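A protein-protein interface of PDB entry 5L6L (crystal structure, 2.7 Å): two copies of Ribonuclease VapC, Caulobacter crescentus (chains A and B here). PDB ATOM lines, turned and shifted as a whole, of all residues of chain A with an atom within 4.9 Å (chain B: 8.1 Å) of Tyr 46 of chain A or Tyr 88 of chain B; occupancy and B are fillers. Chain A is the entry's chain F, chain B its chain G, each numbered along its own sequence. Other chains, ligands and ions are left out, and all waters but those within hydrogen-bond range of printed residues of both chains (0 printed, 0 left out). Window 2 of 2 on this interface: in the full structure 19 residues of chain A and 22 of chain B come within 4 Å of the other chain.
NE of Arg 80 of chain B sits at hydrogen-bond distance from OH of Tyr 46 of chain A, at 3.4 Å.
The side-chain hydroxyl of Tyr 46 of chain A sits at hydrogen-bond distance from the side-chain carboxylate of Glu 84 of chain B, 3.2 Å away.
The guanidinium group (NE) of Arg 80 of chain B sits close to the guanidinium group (NH1) of Arg 56 of chain A, 3.3 Å away.
OE1 of Glu 42 of chain A is in salt-bridge range of NH2 of Arg 56 of chain A (2.8 Å).
The side-chain hydroxyl (OH) of Tyr 46 of chain A sits at hydrogen-bond distance from the guanidinium group (NH1) of Arg 56 of chain A, 3.1 Å away.
The guanidinium group (NE) of Arg 80 of chain B lies within salt-bridge range of the side-chain carboxylate (OE2) of Glu 84 of chain B (3.6 Å).
Glu 42 of chain A touches Arg 80 of chain B.
Tyr 88 of chain B touches Gly 43 of chain A.
Tyr 46 of chain A touches Val 83 of chain B (CD2 to CG2, 3.8 Å).
Tyr 88 of chain B touches Tyr 46 of chain A.
Arg 47 of chain A touches Tyr 88 of chain B (NE to CE2, 3.7 Å).
Of chain B, only Arg 80 (3.4 Å), Val 83 (3.8 Å), Glu 84 (3.2 Å) and Tyr 88 (3.9 Å) come within 4 Å of Tyr 46 of chain A.
Tyr 88 of chain B touches three residues of chain A.
Printed residues of chain A within 4 Å of Glu 84 of chain B: Tyr 46 (3.2 Å).
Of the printed residues of chain B, Arg 47 of chain A touches Tyr 88 (3.7 Å).
Of the printed residues of chain B, Gly 43 of chain A touches Tyr 88.
Of the printed residues of chain B, Glu 42 of chain A touches Arg 80 (3.6 Å).
Arg 96 of chain B touches none of the printed residues of chain A.
The nearest residue of chain A that does not touch Tyr 88 of chain B is Gly 44 of chain A (4.7 Å).
The nearest printed residue of chain A that does not touch Arg 80 of chain B is Val 45 of chain A (6.4 Å).
Hydrophobic or aromatic side chains of chain A that line the printed part of chain B: Tyr 46.
Hydrophobic or aromatic side chains of chain B within 4 Å of the printed part of chain A: Val 83 and Tyr 88.
Along chain B the printed residues that touch a printed residue of chain A span positions 80 to 88.
Among the printed residues, 8 pairs touch across the chains.
No position is printed for both chains.
Of the 8 pairs that touch across the chains among the printed residues, none has its exchanged pair printed and touching as well.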
ATOM      1  N   GLU A  42      21.717   8.196   6.426  1.00  0.00           N
ATOM      2  CA  GLU A  42      21.395   6.841   6.871  1.00  0.00           C
ATOM      3  C   GLU A  42      22.584   6.179   7.554  1.00  0.00           C
ATOM      4  O   GLU A  42      22.405   5.392   8.491  1.00  0.00           O
ATOM      5  CB  GLU A  42      20.922   5.983   5.695  1.00  0.00           C
ATOM      6  CG  GLU A  42      19.583   6.365   5.103  1.00  0.00           C
ATOM      7  CD  GLU A  42      18.394   5.908   5.932  1.00  0.00           C
ATOM      8  OE1 GLU A  42      18.592   5.448   7.084  1.00  0.00           O
ATOM      9  OE2 GLU A  42      17.249   6.011   5.425  1.00  0.00           O
ATOM     10  N   GLY A  43      23.805   6.472   7.088  1.00  0.00           N
ATOM     11  CA  GLY A  43      24.992   5.941   7.739  1.00  0.00           C
ATOM     12  C   GLY A  43      25.288   6.598   9.076  1.00  0.00           C
ATOM     13  O   GLY A  43      25.742   5.930  10.011  1.00  0.00           O
ATOM     14  N   GLY A  44      25.022   7.903   9.195  1.00  0.00           N
ATOM     15  CA  GLY A  44      25.248   8.586  10.450  1.00  0.00           C
ATOM     16  C   GLY A  44      24.379   8.077  11.589  1.00  0.00           C
ATOM     17  O   GLY A  44      24.704   8.297  12.766  1.00  0.00           O
ATOM     18  N   VAL A  45      23.277   7.404  11.272  1.00  0.00           N
ATOM     19  CA  VAL A  45      22.428   6.902  12.336  1.00  0.00           C
ATOM     20  C   VAL A  45      23.157   5.827  13.121  1.00  0.00           C
ATOM     21  O   VAL A  45      22.976   5.709  14.334  1.00  0.00           O
ATOM     22  CB  VAL A  45      21.097   6.401  11.749  1.00  0.00           C
ATOM     23  CG1 VAL A  45      20.271   5.722  12.803  1.00  0.00           C
ATOM     24  CG2 VAL A  45      20.331   7.578  11.132  1.00  0.00           C
ATOM     25  N   TYR A  46      24.047   5.080  12.468  1.00  0.00           N
ATOM     26  CA  TYR A  46      24.733   3.960  13.090  1.00  0.00           C
ATOM     27  C   TYR A  46      26.223   4.230  13.271  1.00  0.00           C
ATOM     28  O   TYR A  46      27.007   3.295  13.453  1.00  0.00           O
ATOM     29  CB  TYR A  46      24.472   2.691  12.278  1.00  0.00           C
ATOM     30  CG  TYR A  46      22.982   2.438  12.111  1.00  0.00           C
ATOM     31  CD1 TYR A  46      22.221   1.928  13.167  1.00  0.00           C
ATOM     32  CD2 TYR A  46      22.324   2.737  10.923  1.00  0.00           C
ATOM     33  CE1 TYR A  46      20.849   1.710  13.046  1.00  0.00           C
ATOM     34  CE2 TYR A  46      20.951   2.521  10.791  1.00  0.00           C
ATOM     35  CZ  TYR A  46      20.220   2.002  11.856  1.00  0.00           C
ATOM     36  OH  TYR A  46      18.858   1.786  11.741  1.00  0.00           O
ATOM     37  N   ARG A  47      26.626   5.496  13.267  1.00  0.00           N
ATOM     38  CA  ARG A  47      28.029   5.794  13.516  1.00  0.00           C
ATOM     39  C   ARG A  47      28.435   5.406  14.933  1.00  0.00           C
ATOM     40  O   ARG A  47      29.523   4.859  15.138  1.00  0.00           O
ATOM     41  CB  ARG A  47      28.312   7.270  13.258  1.00  0.00           C
ATOM     42  CG  ARG A  47      29.780   7.567  13.214  1.00  0.00           C
ATOM     43  CD  ARG A  47      30.074   8.923  12.612  1.00  0.00           C
ATOM     44  NE  ARG A  47      31.209   8.824  11.704  1.00  0.00           N
ATOM     45  CZ  ARG A  47      31.738   9.844  11.047  1.00  0.00           C
ATOM     46  NH1 ARG A  47      31.233  11.059  11.210  1.00  0.00           N
ATOM     47  NH2 ARG A  47      32.772   9.647  10.229  1.00  0.00           N
ATOM     48  N   GLU A  48      27.585   5.678  15.924  1.00  0.00           N
ATOM     49  CA  GLU A  48      27.864   5.334  17.313  1.00  0.00           C
ATOM     50  C   GLU A  48      26.870   4.305  17.829  1.00  0.00           C
ATOM     51  O   GLU A  48      25.744   4.184  17.337  1.00  0.00           O
ATOM     52  CB  GLU A  48      27.807   6.556  18.226  1.00  0.00           C
ATOM     53  CG  GLU A  48      28.771   7.654  17.903  1.00  0.00           C
ATOM     54  CD  GLU A  48      28.620   8.806  18.872  1.00  0.00           C
ATOM     55  OE1 GLU A  48      28.115   8.564  19.996  1.00  0.00           O
ATOM     56  OE2 GLU A  48      28.989   9.950  18.510  1.00  0.00           O
ATOM     57  N   ALA A  52      21.539   5.969  18.528  1.00  0.00           N
ATOM     58  CA  ALA A  52      20.833   5.561  17.320  1.00  0.00           C
ATOM     59  C   ALA A  52      19.370   5.353  17.682  1.00  0.00           C
ATOM     60  O   ALA A  52      19.041   5.151  18.859  1.00  0.00           O
ATOM     61  CB  ALA A  52      21.430   4.281  16.728  1.00  0.00           C
ATOM     62  N   ARG A  56      17.699   7.969  14.499  1.00  0.00           N
ATOM     63  CA  ARG A  56      16.792   7.370  13.530  1.00  0.00           C
ATOM     64  C   ARG A  56      15.420   8.015  13.600  1.00  0.00           C
ATOM     65  O   ARG A  56      14.753   8.202  12.575  1.00  0.00           O
ATOM     66  CB  ARG A  56      16.691   5.868  13.772  1.00  0.00           C
ATOM     67  CG  ARG A  56      15.328   5.266  13.489  1.00  0.00           C
ATOM     68  CD  ARG A  56      15.347   4.464  12.195  1.00  0.00           C
ATOM     69  NE  ARG A  56      15.615   5.289  11.022  1.00  0.00           N
ATOM     70  CZ  ARG A  56      16.759   5.275  10.341  1.00  0.00           C
ATOM     71  NH1 ARG A  56      17.748   4.467  10.703  1.00  0.00           N
ATOM     72  NH2 ARG A  56      16.905   6.058   9.280  1.00  0.00           N
ATOM     73  N   TYR B  79      20.663  -0.008   1.457  1.00  0.00           N
ATOM     74  CA  TYR B  79      21.880   0.562   2.031  1.00  0.00           C
ATOM     75  C   TYR B  79      21.766   0.674   3.545  1.00  0.00           C
ATOM     76  O   TYR B  79      22.719   0.362   4.264  1.00  0.00           O
ATOM     77  CB  TYR B  79      22.199   1.931   1.444  1.00  0.00           C
ATOM     78  CG  TYR B  79      23.392   2.517   2.123  1.00  0.00           C
ATOM     79  CD1 TYR B  79      24.684   2.201   1.692  1.00  0.00           C
ATOM     80  CD2 TYR B  79      23.248   3.371   3.206  1.00  0.00           C
ATOM     81  CE1 TYR B  79      25.802   2.727   2.325  1.00  0.00           C
ATOM     82  CE2 TYR B  79      24.340   3.893   3.855  1.00  0.00           C
ATOM     83  CZ  TYR B  79      25.629   3.578   3.426  1.00  0.00           C
ATOM     84  OH  TYR B  79      26.719   4.140   4.093  1.00  0.00           O
ATOM     85  N   ARG B  80      20.617   1.142   4.047  1.00  0.00           N
ATOM     86  CA  ARG B  80      20.413   1.191   5.492  1.00  0.00           C
ATOM     87  C   ARG B  80      20.487  -0.202   6.092  1.00  0.00           C
ATOM     88  O   ARG B  80      21.048  -0.385   7.180  1.00  0.00           O
ATOM     89  CB  ARG B  80      19.065   1.851   5.836  1.00  0.00           C
ATOM     90  CG  ARG B  80      18.579   1.603   7.271  1.00  0.00           C
ATOM     91  CD  ARG B  80      17.179   2.165   7.586  1.00  0.00           C
ATOM     92  NE  ARG B  80      16.833   1.842   8.979  1.00  0.00           N
ATOM     93  CZ  ARG B  80      15.613   1.890   9.529  1.00  0.00           C
ATOM     94  NH1 ARG B  80      14.538   2.253   8.832  1.00  0.00           N
ATOM     95  NH2 ARG B  80      15.466   1.557  10.802  1.00  0.00           N
ATOM     96  N   ARG B  81      19.936  -1.201   5.394  1.00  0.00           N
ATOM     97  CA  ARG B  81      20.017  -2.563   5.907  1.00  0.00           C
ATOM     98  C   ARG B  81      21.463  -3.008   6.035  1.00  0.00           C
ATOM     99  O   ARG B  81      21.823  -3.703   6.990  1.00  0.00           O
ATOM    100  CB  ARG B  81      19.253  -3.521   5.010  1.00  0.00           C
ATOM    101  CG  ARG B  81      18.656  -4.668   5.761  1.00  0.00           C
ATOM    102  CD  ARG B  81      18.054  -5.666   4.808  1.00  0.00           C
ATOM    103  NE  ARG B  81      18.968  -6.776   4.632  1.00  0.00           N
ATOM    104  CZ  ARG B  81      19.607  -7.043   3.505  1.00  0.00           C
ATOM    105  NH1 ARG B  81      20.435  -8.068   3.448  1.00  0.00           N
ATOM    106  NH2 ARG B  81      19.412  -6.299   2.440  1.00  0.00           N
ATOM    107  N   ILE B  82      22.313  -2.597   5.089  1.00  0.00           N
ATOM    108  CA  ILE B  82      23.712  -3.004   5.112  1.00  0.00           C
ATOM    109  C   ILE B  82      24.430  -2.407   6.319  1.00  0.00           C
ATOM    110  O   ILE B  82      25.081  -3.126   7.087  1.00  0.00           O
ATOM    111  CB  ILE B  82      24.398  -2.617   3.789  1.00  0.00           C
ATOM    112  CG1 ILE B  82      23.911  -3.528   2.649  1.00  0.00           C
ATOM    113  CG2 ILE B  82      25.941  -2.618   3.946  1.00  0.00           C
ATOM    114  CD1 ILE B  82      24.463  -3.165   1.241  1.00  0.00           C
ATOM    115  N   VAL B  83      24.330  -1.085   6.506  1.00  0.00           N
ATOM    116  CA  VAL B  83      25.063  -0.444   7.599  1.00  0.00           C
ATOM    117  C   VAL B  83      24.576  -0.969   8.951  1.00  0.00           C
ATOM    118  O   VAL B  83      25.379  -1.219   9.860  1.00  0.00           O
ATOM    119  CB  VAL B  83      24.965   1.095   7.505  1.00  0.00           C
ATOM    120  CG1 VAL B  83      25.632   1.617   6.233  1.00  0.00           C
ATOM    121  CG2 VAL B  83      23.534   1.548   7.547  1.00  0.00           C
ATOM    122  N   GLU B  84      23.260  -1.166   9.092  1.00  0.00           N
ATOM    123  CA  GLU B  84      22.699  -1.728  10.315  1.00  0.00           C
ATOM    124  C   GLU B  84      23.313  -3.082  10.646  1.00  0.00           C
ATOM    125  O   GLU B  84      23.615  -3.364  11.814  1.00  0.00           O
ATOM    126  CB  GLU B  84      21.185  -1.857  10.175  1.00  0.00           C
ATOM    127  CG  GLU B  84      20.475  -1.782  11.483  1.00  0.00           C
ATOM    128  CD  GLU B  84      18.973  -1.620  11.333  1.00  0.00           C
ATOM    129  OE1 GLU B  84      18.259  -2.032  12.286  1.00  0.00           O
ATOM    130  OE2 GLU B  84      18.517  -1.083  10.280  1.00  0.00           O
ATOM    131  N   SER B  85      23.523  -3.931   9.634  1.00  0.00           N
ATOM    132  CA  SER B  85      24.108  -5.244   9.899  1.00  0.00           C
ATOM    133  C   SER B  85      25.622  -5.186  10.081  1.00  0.00           C
ATOM    134  O   SER B  85      26.156  -5.829  10.995  1.00  0.00           O
ATOM    135  CB  SER B  85      23.777  -6.221   8.780  1.00  0.00           C
ATOM    136  OG  SER B  85      24.757  -7.244   8.741  1.00  0.00           O
ATOM    137  N   ALA B  86      26.336  -4.437   9.231  1.00  0.00           N
ATOM    138  CA  ALA B  86      27.793  -4.481   9.243  1.00  0.00           C
ATOM    139  C   ALA B  86      28.442  -3.355  10.032  1.00  0.00           C
ATOM    140  O   ALA B  86      29.592  -3.504  10.454  1.00  0.00           O
ATOM    141  CB  ALA B  86      28.341  -4.455   7.814  1.00  0.00           C
ATOM    142  N   GLY B  87      27.744  -2.256  10.257  1.00  0.00           N
ATOM    143  CA  GLY B  87      28.384  -1.101  10.851  1.00  0.00           C
ATOM    144  C   GLY B  87      28.701  -0.063   9.795  1.00  0.00           C
ATOM    145  O   GLY B  87      28.873  -0.375   8.611  1.00  0.00           O
ATOM    146  N   TYR B  88      28.751   1.201  10.221  1.00  0.00           N
ATOM    147  CA  TYR B  88      29.032   2.299   9.303  1.00  0.00           C
ATOM    148  C   TYR B  88      30.510   2.324   8.963  1.00  0.00           C
ATOM    149  O   TYR B  88      31.364   2.018   9.801  1.00  0.00           O
ATOM    150  CB  TYR B  88      28.634   3.643   9.908  1.00  0.00           C
ATOM    151  CG  TYR B  88      29.056   4.813   9.059  1.00  0.00           C
ATOM    152  CD1 TYR B  88      28.501   5.005   7.791  1.00  0.00           C
ATOM    153  CD2 TYR B  88      30.011   5.719   9.507  1.00  0.00           C
ATOM    154  CE1 TYR B  88      28.884   6.072   6.990  1.00  0.00           C
ATOM    155  CE2 TYR B  88      30.400   6.801   8.714  1.00  0.00           C
ATOM    156  CZ  TYR B  88      29.834   6.970   7.455  1.00  0.00           C
ATOM    157  OH  TYR B  88      30.211   8.020   6.650  1.00  0.00           O
ATOM    158  N   SER B  89      30.806   2.669   7.716  1.00  0.00           N
ATOM    159  CA  SER B  89      32.188   2.758   7.265  1.00  0.00           C
ATOM    160  C   SER B  89      32.221   3.802   6.169  1.00  0.00           C
ATOM    161  O   SER B  89      31.740   3.535   5.075  1.00  0.00           O
ATOM    162  CB  SER B  89      32.694   1.411   6.752  1.00  0.00           C
ATOM    163  OG  SER B  89      33.825   1.575   5.904  1.00  0.00           O
ATOM    164  N   ARG B  90      32.797   4.964   6.455  1.00  0.00           N
ATOM    165  CA  ARG B  90      32.911   5.991   5.428  1.00  0.00           C
ATOM    166  C   ARG B  90      33.595   5.458   4.168  1.00  0.00           C
ATOM    167  O   ARG B  90      33.151   5.754   3.054  1.00  0.00           O
ATOM    168  CB  ARG B  90      33.656   7.199   5.982  1.00  0.00           C
ATOM    169  CG  ARG B  90      33.382   8.473   5.222  1.00  0.00           C
ATOM    170  CD  ARG B  90      33.830   9.687   6.013  1.00  0.00           C
ATOM    171  NE  ARG B  90      35.255   9.637   6.349  1.00  0.00           N
ATOM    172  CZ  ARG B  90      36.248   9.677   5.461  1.00  0.00           C
ATOM    173  NH1 ARG B  90      35.997   9.748   4.161  1.00  0.00           N
ATOM    174  NH2 ARG B  90      37.506   9.641   5.874  1.00  0.00           N
ATOM    175  N   ARG B  91      34.654   4.643   4.323  1.00  0.00           N
ATOM    176  CA  ARG B  91      35.369   4.117   3.158  1.00  0.00           C
ATOM    177  C   ARG B  91      34.472   3.283   2.244  1.00  0.00           C
ATOM    178  O   ARG B  91      34.568   3.377   1.017  1.00  0.00           O
ATOM    179  CB  ARG B  91      36.577   3.277   3.583  1.00  0.00           C
ATOM    180  CG  ARG B  91      37.287   2.637   2.372  1.00  0.00           C
ATOM    181  CD  ARG B  91      38.537   1.815   2.700  1.00  0.00           C
ATOM    182  NE  ARG B  91      38.270   0.537   3.377  1.00  0.00           N
ATOM    183  CZ  ARG B  91      37.906  -0.596   2.768  1.00  0.00           C
ATOM    184  NH1 ARG B  91      37.732  -0.630   1.446  1.00  0.00           N
ATOM    185  NH2 ARG B  91      37.712  -1.700   3.488  1.00  0.00           N
ATOM    186  N   LYS B  92      33.601   2.455   2.808  1.00  0.00           N
ATOM    187  CA  LYS B  92      32.867   1.479   2.012  1.00  0.00           C
ATOM    188  C   LYS B  92      31.560   1.994   1.437  1.00  0.00           C
ATOM    189  O   LYS B  92      30.822   1.188   0.869  1.00  0.00           O
ATOM    190  CB  LYS B  92      32.566   0.229   2.824  1.00  0.00           C
ATOM    191  CG  LYS B  92      33.784  -0.500   3.323  1.00  0.00           C
ATOM    192  CD  LYS B  92      33.503  -1.976   3.300  1.00  0.00           C
ATOM    193  CE  LYS B  92      34.465  -2.756   4.136  1.00  0.00           C
ATOM    194  NZ  LYS B  92      34.184  -4.194   3.881  1.00  0.00           N
ATOM    195  N   VAL B  93      31.261   3.295   1.525  1.00  0.00           N
ATOM    196  CA  VAL B  93      29.926   3.760   1.154  1.00  0.00           C
ATOM    197  C   VAL B  93      29.642   3.481  -0.321  1.00  0.00           C
ATOM    198  O   VAL B  93      28.608   2.890  -0.649  1.00  0.00           O
ATOM    199  CB  VAL B  93      29.741   5.250   1.496  1.00  0.00           C
ATOM    200  CG1 VAL B  93      28.382   5.714   1.045  1.00  0.00           C
ATOM    201  CG2 VAL B  93      29.872   5.492   2.978  1.00  0.00           C
ATOM    202  N   ARG B  96      29.068  -0.118  -1.087  1.00  0.00           N
ATOM    203  CA  ARG B  96      27.819  -0.589  -0.502  1.00  0.00           C
ATOM    204  C   ARG B  96      26.608  -0.018  -1.238  1.00  0.00           C
ATOM    205  O   ARG B  96      25.600  -0.715  -1.399  1.00  0.00           O
ATOM    206  CB  ARG B  96      27.767  -0.246   0.981  1.00  0.00           C
ATOM    207  CG  ARG B  96      28.558  -1.177   1.831  1.00  0.00           C
ATOM    208  CD  ARG B  96      28.811  -0.596   3.185  1.00  0.00           C
ATOM    209  NE  ARG B  96      29.482  -1.577   4.029  1.00  0.00           N
ATOM    210  CZ  ARG B  96      29.778  -1.389   5.315  1.00  0.00           C
ATOM    211  NH1 ARG B  96      29.455  -0.244   5.912  1.00  0.00           N
ATOM    212  NH2 ARG B  96      30.399  -2.348   6.004  1.00  0.00           N
